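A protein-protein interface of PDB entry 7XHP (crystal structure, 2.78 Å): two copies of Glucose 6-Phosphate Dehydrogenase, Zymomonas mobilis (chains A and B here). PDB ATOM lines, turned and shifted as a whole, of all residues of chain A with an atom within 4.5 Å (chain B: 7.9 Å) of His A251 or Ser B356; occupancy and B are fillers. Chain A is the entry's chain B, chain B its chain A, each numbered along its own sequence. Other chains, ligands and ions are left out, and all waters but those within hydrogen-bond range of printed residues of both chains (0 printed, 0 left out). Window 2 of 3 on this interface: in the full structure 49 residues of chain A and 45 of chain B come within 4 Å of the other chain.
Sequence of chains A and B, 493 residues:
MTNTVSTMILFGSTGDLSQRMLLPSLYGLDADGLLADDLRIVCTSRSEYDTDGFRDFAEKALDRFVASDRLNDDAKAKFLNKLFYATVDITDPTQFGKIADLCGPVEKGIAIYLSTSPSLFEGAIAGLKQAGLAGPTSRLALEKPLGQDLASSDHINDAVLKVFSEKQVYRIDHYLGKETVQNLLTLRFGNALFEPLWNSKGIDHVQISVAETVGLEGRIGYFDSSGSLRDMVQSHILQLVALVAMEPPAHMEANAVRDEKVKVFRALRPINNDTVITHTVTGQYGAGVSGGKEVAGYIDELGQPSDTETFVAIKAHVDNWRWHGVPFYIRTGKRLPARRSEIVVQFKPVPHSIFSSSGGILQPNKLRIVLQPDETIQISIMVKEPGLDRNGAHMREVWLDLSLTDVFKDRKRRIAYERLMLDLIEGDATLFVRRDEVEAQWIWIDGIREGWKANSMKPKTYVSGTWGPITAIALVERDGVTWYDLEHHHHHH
Hydrophobic or aromatic side chains of chain B that line the printed part of chain A: His B352, Ile B354 and Phe B355.
Hydrophobic or aromatic side chains of chain A that line the printed part of chain B: Pro A249, His A251 and Met A252.
Among the printed residues, 6 pairs touch across the chains.
Among the printed residues, merely in contact across the chains: Pro A249 with Ile B354, His A251 with Ile B354 and Met A252 with Phe B355.
No position is printed for both chains.
Of the 6 pairs that touch across the chains among the printed residues, none has its exchanged pair printed and touching as well.
The backbone carbonyl oxygen (O) of Ala A250 is in hydrogen-bond range of a ring nitrogen (NE2) of His B352.
N of Met A252 is in hydrogen-bond range of O of Ile B354, 3.1 Å away.
O of Ser B356 is in hydrogen-bond range of NE2 of His A251, 2.9 Å away.
His A251 touches two residues of chain B.
Of the printed residues of chain B, Met A252 touches Ile B354 (3.1 Å) and Phe B355 (3.5 Å).
Of the printed residues of chain A, His B352 touches Ala A250 (3.3 Å).
Of the printed residues of chain A, Ile B354 touches Pro A249 (3.7 Å), His A251 (3.5 Å) and Met A252 (3.1 Å).
Of chain A, only His A251 comes within 4 Å of Ser B356.
The nearest printed residue of chain A that does not touch Ile B354 is Ala A250 (4.3 Å).
The backbone carbonyl oxygen (O) of Ser B353 sits at hydrogen-bond distance from the side-chain hydroxyl (OG) of Ser B356 (3.2 Å).
The side-chain hydroxyl (OG) of Ser B357 sits at hydrogen-bond distance from the backbone carbonyl oxygen (O) of Phe B355 (2.9 Å).
The backbone carbonyl oxygen of Phe B355 sits close to the backbone NH of Gly B360 (3.0 Å).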
ATOM      1  N   PRO A 249     -25.220  24.655  -3.803  1.00  0.00           N
ATOM      2  CA  PRO A 249     -24.396  23.598  -3.214  1.00  0.00           C
ATOM      3  C   PRO A 249     -22.924  23.992  -3.394  1.00  0.00           C
ATOM      4  O   PRO A 249     -22.642  24.776  -4.275  1.00  0.00           O
ATOM      5  CB  PRO A 249     -24.755  22.366  -4.047  1.00  0.00           C
ATOM      6  CG  PRO A 249     -25.133  22.933  -5.392  1.00  0.00           C
ATOM      7  CD  PRO A 249     -25.822  24.243  -5.074  1.00  0.00           C
ATOM      8  N   ALA A 250     -22.028  23.452  -2.569  1.00  0.00           N
ATOM      9  CA  ALA A 250     -20.588  23.751  -2.736  1.00  0.00           C
ATOM     10  C   ALA A 250     -20.140  23.253  -4.108  1.00  0.00           C
ATOM     11  O   ALA A 250     -19.344  23.951  -4.755  1.00  0.00           O
ATOM     12  CB  ALA A 250     -19.802  23.097  -1.637  1.00  0.00           C
ATOM     13  N   HIS A 251     -20.612  22.080  -4.522  1.00  0.00           N
ATOM     14  CA  HIS A 251     -20.320  21.577  -5.889  1.00  0.00           C
ATOM     15  C   HIS A 251     -21.583  20.931  -6.461  1.00  0.00           C
ATOM     16  O   HIS A 251     -22.449  20.539  -5.667  1.00  0.00           O
ATOM     17  CB  HIS A 251     -19.093  20.660  -5.924  1.00  0.00           C
ATOM     18  CG  HIS A 251     -18.311  20.842  -7.180  1.00  0.00           C
ATOM     19  ND1 HIS A 251     -16.976  21.182  -7.177  1.00  0.00           N
ATOM     20  CD2 HIS A 251     -18.684  20.772  -8.476  1.00  0.00           C
ATOM     21  CE1 HIS A 251     -16.553  21.291  -8.419  1.00  0.00           C
ATOM     22  NE2 HIS A 251     -17.583  21.045  -9.234  1.00  0.00           N
ATOM     23  N   MET A 252     -21.676  20.822  -7.786  1.00  0.00           N
ATOM     24  CA  MET A 252     -22.942  20.313  -8.357  1.00  0.00           C
ATOM     25  C   MET A 252     -22.892  18.790  -8.448  1.00  0.00           C
ATOM     26  O   MET A 252     -22.265  18.262  -9.377  1.00  0.00           O
ATOM     27  CB  MET A 252     -23.149  20.880  -9.763  1.00  0.00           C
ATOM     28  CG  MET A 252     -23.934  22.163  -9.788  1.00  0.00           C
ATOM     29  SD  MET A 252     -25.698  21.869  -9.999  1.00  0.00           S
ATOM     30  CE  MET A 252     -25.780  21.589 -11.766  1.00  0.00           C
ATOM     31  N   GLU A 253     -23.607  18.124  -7.550  1.00  0.00           N
ATOM     32  CA  GLU A 253     -23.749  16.652  -7.576  1.00  0.00           C
ATOM     33  C   GLU A 253     -25.208  16.453  -7.197  1.00  0.00           C
ATOM     34  O   GLU A 253     -25.759  17.346  -6.540  1.00  0.00           O
ATOM     35  CB  GLU A 253     -22.773  15.926  -6.650  1.00  0.00           C
ATOM     36  CG  GLU A 253     -22.400  16.671  -5.387  1.00  0.00           C
ATOM     37  CD  GLU A 253     -21.659  15.784  -4.400  1.00  0.00           C
ATOM     38  OE1 GLU A 253     -22.017  14.596  -4.297  1.00  0.00           O
ATOM     39  OE2 GLU A 253     -20.721  16.277  -3.749  1.00  0.00           O
ATOM     40  N   ALA A 256     -25.520  16.889  -3.399  1.00  0.00           N
ATOM     41  CA  ALA A 256     -25.373  18.267  -2.871  1.00  0.00           C
ATOM     42  C   ALA A 256     -26.515  19.199  -3.300  1.00  0.00           C
ATOM     43  O   ALA A 256     -27.014  19.949  -2.451  1.00  0.00           O
ATOM     44  CB  ALA A 256     -24.037  18.830  -3.278  1.00  0.00           C
ATOM     45  N   HIS B 352     -17.184  31.683  -7.096  1.00  0.00           N
ATOM     46  CA  HIS B 352     -17.020  30.241  -7.198  1.00  0.00           C
ATOM     47  C   HIS B 352     -17.851  29.731  -8.360  1.00  0.00           C
ATOM     48  O   HIS B 352     -19.032  30.070  -8.470  1.00  0.00           O
ATOM     49  CB  HIS B 352     -17.476  29.591  -5.882  1.00  0.00           C
ATOM     50  CG  HIS B 352     -17.017  28.179  -5.688  1.00  0.00           C
ATOM     51  ND1 HIS B 352     -15.700  27.845  -5.456  1.00  0.00           N
ATOM     52  CD2 HIS B 352     -17.715  27.020  -5.623  1.00  0.00           C
ATOM     53  CE1 HIS B 352     -15.601  26.540  -5.288  1.00  0.00           C
ATOM     54  NE2 HIS B 352     -16.809  26.015  -5.385  1.00  0.00           N
ATOM     55  N   SER B 353     -17.253  28.899  -9.204  1.00  0.00           N
ATOM     56  CA  SER B 353     -18.024  28.213 -10.232  1.00  0.00           C
ATOM     57  C   SER B 353     -18.483  26.915  -9.589  1.00  0.00           C
ATOM     58  O   SER B 353     -17.717  25.955  -9.485  1.00  0.00           O
ATOM     59  CB  SER B 353     -17.185  27.968 -11.480  1.00  0.00           C
ATOM     60  OG  SER B 353     -18.003  27.686 -12.601  1.00  0.00           O
ATOM     61  N   ILE B 354     -19.748  26.875  -9.167  1.00  0.00           N
ATOM     62  CA  ILE B 354     -20.267  25.667  -8.543  1.00  0.00           C
ATOM     63  C   ILE B 354     -20.482  24.565  -9.561  1.00  0.00           C
ATOM     64  O   ILE B 354     -20.817  23.436  -9.187  1.00  0.00           O
ATOM     65  CB  ILE B 354     -21.579  25.945  -7.779  1.00  0.00           C
ATOM     66  CG1 ILE B 354     -22.780  25.909  -8.720  1.00  0.00           C
ATOM     67  CG2 ILE B 354     -21.506  27.289  -7.084  1.00  0.00           C
ATOM     68  CD1 ILE B 354     -23.931  25.066  -8.208  1.00  0.00           C
ATOM     69  N   PHE B 355     -20.273  24.869 -10.841  1.00  0.00           N
ATOM     70  CA  PHE B 355     -20.425  23.918 -11.929  1.00  0.00           C
ATOM     71  C   PHE B 355     -19.072  23.502 -12.483  1.00  0.00           C
ATOM     72  O   PHE B 355     -18.912  23.309 -13.686  1.00  0.00           O
ATOM     73  CB  PHE B 355     -21.284  24.500 -13.047  1.00  0.00           C
ATOM     74  CG  PHE B 355     -22.532  25.157 -12.563  1.00  0.00           C
ATOM     75  CD1 PHE B 355     -22.547  26.505 -12.248  1.00  0.00           C
ATOM     76  CD2 PHE B 355     -23.693  24.427 -12.414  1.00  0.00           C
ATOM     77  CE1 PHE B 355     -23.697  27.104 -11.797  1.00  0.00           C
ATOM     78  CE2 PHE B 355     -24.841  25.018 -11.958  1.00  0.00           C
ATOM     79  CZ  PHE B 355     -24.849  26.352 -11.648  1.00  0.00           C
ATOM     80  N   SER B 356     -18.091  23.387 -11.583  1.00  0.00           N
ATOM     81  CA  SER B 356     -16.731  22.945 -11.985  1.00  0.00           C
ATOM     82  C   SER B 356     -16.790  21.455 -12.313  1.00  0.00           C
ATOM     83  O   SER B 356     -16.054  20.676 -11.685  1.00  0.00           O
ATOM     84  CB  SER B 356     -15.704  23.258 -10.927  1.00  0.00           C
ATOM     85  OG  SER B 356     -15.243  24.594 -11.050  1.00  0.00           O
ATOM     86  N   SER B 357     -17.596  21.099 -13.306  1.00  0.00           N
ATOM     87  CA  SER B 357     -17.776  19.693 -13.736  1.00  0.00           C
ATOM     88  C   SER B 357     -16.776  19.491 -14.863  1.00  0.00           C
ATOM     89  O   SER B 357     -16.901  18.472 -15.558  1.00  0.00           O
ATOM     90  CB  SER B 357     -19.190  19.455 -14.175  1.00  0.00           C
ATOM     91  OG  SER B 357     -19.910  20.677 -14.265  1.00  0.00           O
ATOM     92  N   SER B 358     -15.884  20.468 -15.061  1.00  0.00           N
ATOM     93  CA  SER B 358     -14.911  20.502 -16.185  1.00  0.00           C
ATOM     94  C   SER B 358     -15.589  21.283 -17.305  1.00  0.00           C
ATOM     95  O   SER B 358     -14.928  21.540 -18.325  1.00  0.00           O
ATOM     96  CB  SER B 358     -14.457  19.134 -16.621  1.00  0.00           C
ATOM     97  OG  SER B 358     -14.058  18.353 -15.505  1.00  0.00           O
ATOM     98  N   GLY B 359     -16.871  21.611 -17.131  1.00  0.00           N
ATOM     99  CA  GLY B 359     -17.551  22.527 -18.065  1.00  0.00           C
ATOM    100  C   GLY B 359     -17.806  23.866 -17.397  1.00  0.00           C
ATOM    101  O   GLY B 359     -18.433  24.726 -18.036  1.00  0.00           O
ATOM    102  N   GLY B 360     -17.351  24.037 -16.152  1.00  0.00           N
ATOM    103  CA  GLY B 360     -17.656  25.264 -15.388  1.00  0.00           C
ATOM    104  C   GLY B 360     -16.715  26.431 -15.620  1.00  0.00           C
ATOM    105  O   GLY B 360     -15.944  26.751 -14.697  1.00  0.00           O
ATOM    106  N   ILE B 361     -16.794  27.069 -16.786  1.00  0.00           N
ATOM    107  CA  ILE B 361     -16.002  28.308 -17.026  1.00  0.00           C
ATOM    108  C   ILE B 361     -17.031  29.413 -17.250  1.00  0.00           C
ATOM    109  O   ILE B 361     -17.890  29.241 -18.135  1.00  0.00           O
ATOM    110  CB  ILE B 361     -15.067  28.141 -18.238  1.00  0.00           C
ATOM    111  N   ASN B 391     -19.587  14.114 -19.151  1.00  0.00           N
ATOM    112  CA  ASN B 391     -18.806  14.132 -17.915  1.00  0.00           C
ATOM    113  C   ASN B 391     -18.638  15.572 -17.428  1.00  0.00           C
ATOM    114  O   ASN B 391     -17.585  15.948 -16.914  1.00  0.00           O
ATOM    115  CB  ASN B 391     -17.450  13.429 -18.057  1.00  0.00           C
ATOM    116  N   GLY B 392     -19.668  16.388 -17.628  1.00  0.00           N
ATOM    117  CA  GLY B 392     -19.673  17.758 -17.145  1.00  0.00           C
ATOM    118  C   GLY B 392     -20.810  18.535 -17.768  1.00  0.00           C
ATOM    119  O   GLY B 392     -21.555  18.029 -18.610  1.00  0.00           O
ATOM    120  N   ALA B 393     -20.982  19.770 -17.287  1.00  0.00           N
ATOM    121  CA  ALA B 393     -21.995  20.661 -17.846  1.00  0.00           C
ATOM    122  C   ALA B 393     -21.334  21.642 -18.804  1.00  0.00           C
ATOM    123  O   ALA B 393     -20.350  22.301 -18.448  1.00  0.00           O
ATOM    124  CB  ALA B 393     -22.775  21.425 -16.775  1.00  0.00           C
ATOM    125  N   MET B 395     -21.998  24.973 -21.381  1.00  0.00           N
ATOM    126  CA  MET B 395     -22.863  26.139 -21.334  1.00  0.00           C
ATOM    127  C   MET B 395     -22.375  27.159 -22.358  1.00  0.00           C
ATOM    128  O   MET B 395     -21.281  27.028 -22.915  1.00  0.00           O
ATOM    129  CB  MET B 395     -22.889  26.678 -19.898  1.00  0.00           C
ATOM    130  CG  MET B 395     -23.566  25.711 -18.923  1.00  0.00           C
ATOM    131  SD  MET B 395     -23.053  25.801 -17.188  1.00  0.00           S
ATOM    132  CE  MET B 395     -21.307  26.151 -17.317  1.00  0.00           C
